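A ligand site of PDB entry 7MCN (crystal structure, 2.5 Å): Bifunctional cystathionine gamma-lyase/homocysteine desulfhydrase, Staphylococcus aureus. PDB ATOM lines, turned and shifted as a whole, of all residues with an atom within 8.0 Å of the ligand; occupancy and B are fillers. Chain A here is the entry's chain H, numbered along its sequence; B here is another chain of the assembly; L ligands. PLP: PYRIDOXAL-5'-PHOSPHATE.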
ATOM      1  N   SER A   1      10.055  16.402 -20.981  1.00  0.00           N
ATOM      2  CA  SER A   1      10.961  17.539 -20.954  1.00  0.00           C
ATOM      3  C   SER A   1      11.910  17.400 -19.767  1.00  0.00           C
ATOM      4  O   SER A   1      12.915  16.727 -19.867  1.00  0.00           O
ATOM      5  CB  SER A   1      10.153  18.841 -20.882  1.00  0.00           C
ATOM      6  OG  SER A   1      10.978  19.958 -20.596  1.00  0.00           O
ATOM      7  N   ASN A   2      11.575  18.006 -18.626  1.00  0.00           N
ATOM      8  CA  ASN A   2      12.318  17.752 -17.400  1.00  0.00           C
ATOM      9  C   ASN A   2      11.991  16.359 -16.856  1.00  0.00           C
ATOM     10  O   ASN A   2      10.983  15.741 -17.233  1.00  0.00           O
ATOM     11  CB  ASN A   2      12.027  18.832 -16.360  1.00  0.00           C
ATOM     12  CG  ASN A   2      12.689  20.142 -16.698  1.00  0.00           C
ATOM     13  OD1 ASN A   2      13.681  20.164 -17.398  1.00  0.00           O
ATOM     14  ND2 ASN A   2      12.129  21.232 -16.207  1.00  0.00           N
ATOM     15  N   LYS A   3      12.858  15.861 -15.965  1.00  0.00           N
ATOM     16  CA  LYS A   3      12.849  14.435 -15.633  1.00  0.00           C
ATOM     17  C   LYS A   3      11.540  14.001 -14.975  1.00  0.00           C
ATOM     18  O   LYS A   3      11.024  12.914 -15.270  1.00  0.00           O
ATOM     19  CB  LYS A   3      14.030  14.088 -14.723  1.00  0.00           C
ATOM     20  CG  LYS A   3      15.354  14.647 -15.184  1.00  0.00           C
ATOM     21  CD  LYS A   3      16.521  13.955 -14.465  1.00  0.00           C
ATOM     22  CE  LYS A   3      16.912  14.697 -13.179  1.00  0.00           C
ATOM     23  NZ  LYS A   3      18.021  14.012 -12.467  1.00  0.00           N
ATOM     24  N   LYS A   4      11.011  14.805 -14.040  1.00  0.00           N
ATOM     25  CA  LYS A   4       9.790  14.393 -13.358  1.00  0.00           C
ATOM     26  C   LYS A   4       8.616  14.309 -14.318  1.00  0.00           C
ATOM     27  O   LYS A   4       7.698  13.506 -14.120  1.00  0.00           O
ATOM     28  CB  LYS A   4       9.469  15.322 -12.203  1.00  0.00           C
ATOM     29  CG  LYS A   4      10.498  15.295 -11.079  1.00  0.00           C
ATOM     30  CD  LYS A   4      10.069  16.193  -9.933  1.00  0.00           C
ATOM     31  CE  LYS A   4      11.245  16.759  -9.191  1.00  0.00           C
ATOM     32  NZ  LYS A   4      10.836  17.620  -8.040  1.00  0.00           N
ATOM     33  N   THR A   5       8.642  15.121 -15.386  1.00  0.00           N
ATOM     34  CA  THR A   5       7.619  15.016 -16.413  1.00  0.00           C
ATOM     35  C   THR A   5       7.801  13.754 -17.239  1.00  0.00           C
ATOM     36  O   THR A   5       6.845  12.995 -17.479  1.00  0.00           O
ATOM     37  CB  THR A   5       7.681  16.250 -17.314  1.00  0.00           C
ATOM     38  OG1 THR A   5       7.596  17.434 -16.508  1.00  0.00           O
ATOM     39  CG2 THR A   5       6.546  16.223 -18.324  1.00  0.00           C
ATOM     40  N   LYS A   6       9.032  13.504 -17.686  1.00  0.00           N
ATOM     41  CA  LYS A   6       9.341  12.334 -18.494  1.00  0.00           C
ATOM     42  C   LYS A   6       8.985  11.048 -17.758  1.00  0.00           C
ATOM     43  O   LYS A   6       8.606  10.053 -18.391  1.00  0.00           O
ATOM     44  CB  LYS A   6      10.829  12.360 -18.848  1.00  0.00           C
ATOM     45  CG  LYS A   6      11.306  11.263 -19.778  1.00  0.00           C
ATOM     46  CD  LYS A   6      12.675  11.610 -20.365  1.00  0.00           C
ATOM     47  CE  LYS A   6      13.539  10.365 -20.561  1.00  0.00           C
ATOM     48  NZ  LYS A   6      14.970  10.699 -20.891  1.00  0.00           N
ATOM     49  N   LEU A   7       9.093  11.056 -16.431  1.00  0.00           N
ATOM     50  CA  LEU A   7       8.729   9.878 -15.654  1.00  0.00           C
ATOM     51  C   LEU A   7       7.243   9.570 -15.757  1.00  0.00           C
ATOM     52  O   LEU A   7       6.851   8.403 -15.709  1.00  0.00           O
ATOM     53  CB  LEU A   7       9.102  10.082 -14.188  1.00  0.00           C
ATOM     54  CG  LEU A   7      10.537   9.728 -13.828  1.00  0.00           C
ATOM     55  CD1 LEU A   7      10.857  10.205 -12.436  1.00  0.00           C
ATOM     56  CD2 LEU A   7      10.721   8.234 -13.929  1.00  0.00           C
ATOM     57  N   ILE A   8       6.424  10.603 -15.926  1.00  0.00           N
ATOM     58  CA  ILE A   8       4.973  10.423 -15.960  1.00  0.00           C
ATOM     59  C   ILE A   8       4.494  10.139 -17.375  1.00  0.00           C
ATOM     60  O   ILE A   8       3.626   9.287 -17.585  1.00  0.00           O
ATOM     61  CB  ILE A   8       4.279  11.671 -15.363  1.00  0.00           C
ATOM     62  CG1 ILE A   8       4.735  11.904 -13.923  1.00  0.00           C
ATOM     63  CG2 ILE A   8       2.777  11.532 -15.424  1.00  0.00           C
ATOM     64  CD1 ILE A   8       4.732  10.658 -13.064  1.00  0.00           C
ATOM     65  N   HIS A   9       5.068  10.827 -18.357  1.00  0.00           N
ATOM     66  CA  HIS A   9       4.568  10.744 -19.718  1.00  0.00           C
ATOM     67  C   HIS A   9       5.475   9.976 -20.669  1.00  0.00           C
ATOM     68  O   HIS A   9       5.089   9.741 -21.811  1.00  0.00           O
ATOM     69  CB  HIS A   9       4.308  12.164 -20.227  1.00  0.00           C
ATOM     70  CG  HIS A   9       3.278  12.883 -19.418  1.00  0.00           C
ATOM     71  ND1 HIS A   9       1.932  12.599 -19.515  1.00  0.00           N
ATOM     72  CD2 HIS A   9       3.401  13.831 -18.448  1.00  0.00           C
ATOM     73  CE1 HIS A   9       1.269  13.355 -18.665  1.00  0.00           C
ATOM     74  NE2 HIS A   9       2.136  14.118 -18.010  1.00  0.00           N
ATOM     75  N   GLY A  10       6.647   9.540 -20.214  1.00  0.00           N
ATOM     76  CA  GLY A  10       7.524   8.758 -21.078  1.00  0.00           C
ATOM     77  C   GLY A  10       7.118   7.297 -21.133  1.00  0.00           C
ATOM     78  O   GLY A  10       6.670   6.715 -20.151  1.00  0.00           O
ATOM     79  N   GLY A  11       7.293   6.700 -22.310  1.00  0.00           N
ATOM     80  CA  GLY A  11       6.861   5.333 -22.533  1.00  0.00           C
ATOM     81  C   GLY A  11       5.372   5.253 -22.831  1.00  0.00           C
ATOM     82  O   GLY A  11       4.625   6.229 -22.752  1.00  0.00           O
ATOM     83  N   THR A  62      12.739   4.255 -22.629  1.00  0.00           N
ATOM     84  CA  THR A  62      12.591   5.712 -22.657  1.00  0.00           C
ATOM     85  C   THR A  62      13.465   6.367 -21.603  1.00  0.00           C
ATOM     86  O   THR A  62      14.163   7.352 -21.883  1.00  0.00           O
ATOM     87  CB  THR A  62      11.121   6.088 -22.454  1.00  0.00           C
ATOM     88  OG1 THR A  62      10.370   5.745 -23.617  1.00  0.00           O
ATOM     89  CG2 THR A  62      10.972   7.574 -22.195  1.00  0.00           C
ATOM     90  N   LEU A  63      13.442   5.824 -20.376  1.00  0.00           N
ATOM     91  CA  LEU A  63      14.094   6.498 -19.261  1.00  0.00           C
ATOM     92  C   LEU A  63      15.611   6.450 -19.372  1.00  0.00           C
ATOM     93  O   LEU A  63      16.306   7.320 -18.829  1.00  0.00           O
ATOM     94  CB  LEU A  63      13.627   5.884 -17.939  1.00  0.00           C
ATOM     95  CG  LEU A  63      12.153   6.137 -17.586  1.00  0.00           C
ATOM     96  CD1 LEU A  63      11.801   5.534 -16.248  1.00  0.00           C
ATOM     97  CD2 LEU A  63      11.854   7.614 -17.610  1.00  0.00           C
ATOM     98  N   GLU A  64      16.146   5.450 -20.080  1.00  0.00           N
ATOM     99  CA  GLU A  64      17.579   5.345 -20.315  1.00  0.00           C
ATOM    100  C   GLU A  64      17.980   5.873 -21.684  1.00  0.00           C
ATOM    101  O   GLU A  64      19.121   5.640 -22.111  1.00  0.00           O
ATOM    102  CB  GLU A  64      18.027   3.881 -20.160  1.00  0.00           C
ATOM    103  CG  GLU A  64      17.989   3.339 -18.735  1.00  0.00           C
ATOM    104  CD  GLU A  64      19.067   3.922 -17.818  1.00  0.00           C
ATOM    105  OE1 GLU A  64      19.650   4.999 -18.137  1.00  0.00           O
ATOM    106  OE2 GLU A  64      19.332   3.311 -16.754  1.00  0.00           O
ATOM    107  N   ASN A  65      17.083   6.560 -22.384  1.00  0.00           N
ATOM    108  CA  ASN A  65      17.305   7.051 -23.755  1.00  0.00           C
ATOM    109  C   ASN A  65      17.845   5.951 -24.669  1.00  0.00           C
ATOM    110  O   ASN A  65      18.713   6.170 -25.515  1.00  0.00           O
ATOM    111  CB  ASN A  65      18.228   8.261 -23.760  1.00  0.00           C
ATOM    112  CG  ASN A  65      17.757   9.334 -22.849  1.00  0.00           C
ATOM    113  OD1 ASN A  65      16.562   9.619 -22.790  1.00  0.00           O
ATOM    114  ND2 ASN A  65      18.691   9.939 -22.120  1.00  0.00           N
ATOM    115  N   ASN A 181      22.705   7.897 -16.844  1.00  0.00           N
ATOM    116  CA  ASN A 181      22.227   7.251 -18.074  1.00  0.00           C
ATOM    117  C   ASN A 181      23.433   6.761 -18.857  1.00  0.00           C
ATOM    118  O   ASN A 181      23.964   7.482 -19.717  1.00  0.00           O
ATOM    119  CB  ASN A 181      21.346   8.195 -18.893  1.00  0.00           C
ATOM    120  CG  ASN A 181      20.170   8.738 -18.090  1.00  0.00           C
ATOM    121  OD1 ASN A 181      20.104   9.920 -17.823  1.00  0.00           O
ATOM    122  ND2 ASN A 181      19.266   7.864 -17.691  1.00  0.00           N
ATOM    123  N   ASP A 184      23.764   7.211 -22.699  1.00  0.00           N
ATOM    124  CA  ASP A 184      24.158   8.526 -23.194  1.00  0.00           C
ATOM    125  C   ASP A 184      25.669   8.704 -23.183  1.00  0.00           C
ATOM    126  O   ASP A 184      26.156   9.667 -23.767  1.00  0.00           O
ATOM    127  CB  ASP A 184      23.553   9.644 -22.350  1.00  0.00           C
ATOM    128  CG  ASP A 184      22.054   9.772 -22.515  1.00  0.00           C
ATOM    129  OD1 ASP A 184      21.503   9.162 -23.469  1.00  0.00           O
ATOM    130  OD2 ASP A 184      21.440  10.487 -21.700  1.00  0.00           O
ATOM    131  N   SER B 316       0.375  20.097 -23.621  1.00  0.00           N
ATOM    132  CA  SER B 316       0.981  18.792 -23.824  1.00  0.00           C
ATOM    133  C   SER B 316       0.914  17.896 -22.591  1.00  0.00           C
ATOM    134  O   SER B 316       0.836  16.671 -22.740  1.00  0.00           O
ATOM    135  CB  SER B 316       2.438  18.948 -24.247  1.00  0.00           C
ATOM    136  OG  SER B 316       2.536  19.783 -25.394  1.00  0.00           O
ATOM    137  N   TYR B 317       0.901  18.468 -21.385  1.00  0.00           N
ATOM    138  CA  TYR B 317       1.001  17.675 -20.163  1.00  0.00           C
ATOM    139  C   TYR B 317      -0.271  17.682 -19.323  1.00  0.00           C
ATOM    140  O   TYR B 317      -0.277  17.115 -18.232  1.00  0.00           O
ATOM    141  CB  TYR B 317       2.181  18.159 -19.321  1.00  0.00           C
ATOM    142  CG  TYR B 317       3.477  18.182 -20.101  1.00  0.00           C
ATOM    143  CD1 TYR B 317       3.885  17.067 -20.804  1.00  0.00           C
ATOM    144  CD2 TYR B 317       4.265  19.321 -20.169  1.00  0.00           C
ATOM    145  CE1 TYR B 317       5.062  17.068 -21.541  1.00  0.00           C
ATOM    146  CE2 TYR B 317       5.440  19.338 -20.899  1.00  0.00           C
ATOM    147  CZ  TYR B 317       5.831  18.206 -21.597  1.00  0.00           C
ATOM    148  OH  TYR B 317       6.992  18.190 -22.328  1.00  0.00           O
ATOM    149  N   ASP B 368       7.629  22.592 -16.108  1.00  0.00           N
ATOM    150  CA  ASP B 368       6.916  22.091 -17.268  1.00  0.00           C
ATOM    151  C   ASP B 368       5.423  22.397 -17.169  1.00  0.00           C
ATOM    152  O   ASP B 368       4.810  22.878 -18.128  1.00  0.00           O
ATOM    153  CB  ASP B 368       7.172  20.597 -17.425  1.00  0.00           C
ATOM    154  CG  ASP B 368       8.548  20.287 -17.967  1.00  0.00           C
ATOM    155  OD1 ASP B 368       9.178  21.198 -18.574  1.00  0.00           O
ATOM    156  OD2 ASP B 368       8.991  19.133 -17.806  1.00  0.00           O
HETATM  157  N1  PLP L   1       9.722  11.825 -23.328  1.00  0.00           N
HETATM  158  C2  PLP L   1       8.709  12.524 -22.808  1.00  0.00           C
HETATM  159  C2A PLP L   1       7.377  11.860 -22.607  1.00  0.00           C
HETATM  160  C3  PLP L   1       8.887  13.876 -22.452  1.00  0.00           C
HETATM  161  O3  PLP L   1       7.839  14.553 -21.939  1.00  0.00           O
HETATM  162  C4  PLP L   1      10.111  14.495 -22.644  1.00  0.00           C
HETATM  163  C4A PLP L   1      10.322  15.905 -22.297  1.00  0.00           C
HETATM  164  C5  PLP L   1      11.171  13.737 -23.188  1.00  0.00           C
HETATM  165  C6  PLP L   1      10.918  12.414 -23.500  1.00  0.00           C
HETATM  166  C5A PLP L   1      12.538  14.326 -23.425  1.00  0.00           C
HETATM  167  O4P PLP L   1      13.539  13.366 -23.134  1.00  0.00           O
HETATM  168  P   PLP L   1      15.063  13.840 -22.995  1.00  0.00           P
HETATM  169  O1P PLP L   1      15.906  12.966 -23.908  1.00  0.00           O
HETATM  170  O2P PLP L   1      15.542  13.674 -21.566  1.00  0.00           O
HETATM  171  O3P PLP L   1      15.107  15.306 -23.368  1.00  0.00           O
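Residues that only touch the ligand: His 9 (3.2 Å), Gly 10 (3.4 Å), Asn 65 (3.6 Å) and Tyr 317 of chain B (3.8 Å). Hydrophobic or aromatic side chains within 4 Å of the ligand: His 9 and Tyr 317 of chain B. Within 4 Å of the ligand: Ser 1, Lys 6, His 9, Gly 10, Asn 65 and Tyr 317 of chain B. The nearest printed residue that does not touch the ligand is Thr 5 (4.2 Å).
The side-chain carboxylate (OD1) of Asp 368 of chain B is in hydrogen-bond range of the side-chain hydroxyl (OG) of Ser 1 (3.0 Å). The side-chain amino group (NZ) of Lys 6 sits at hydrogen-bond distance from the side-chain amide oxygen (OD1) of Asn 65. OD1 of Asn 65 lies close to O of Thr 62, 3.4 Å away. The side-chain amide nitrogen (ND2) of Asn 65 lies within hydrogen-bond range of the side-chain carboxylate (OD2) of Asp 184, at 2.8 Å.
The backbone NH of Ser 1 is bonded to a carbon (C4A) of the ligand (1.4 Å). The side-chain amino group (NZ) of Lys 6 lies within salt-bridge range of an oxygen (O2P) of the ligand (3.1 Å).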
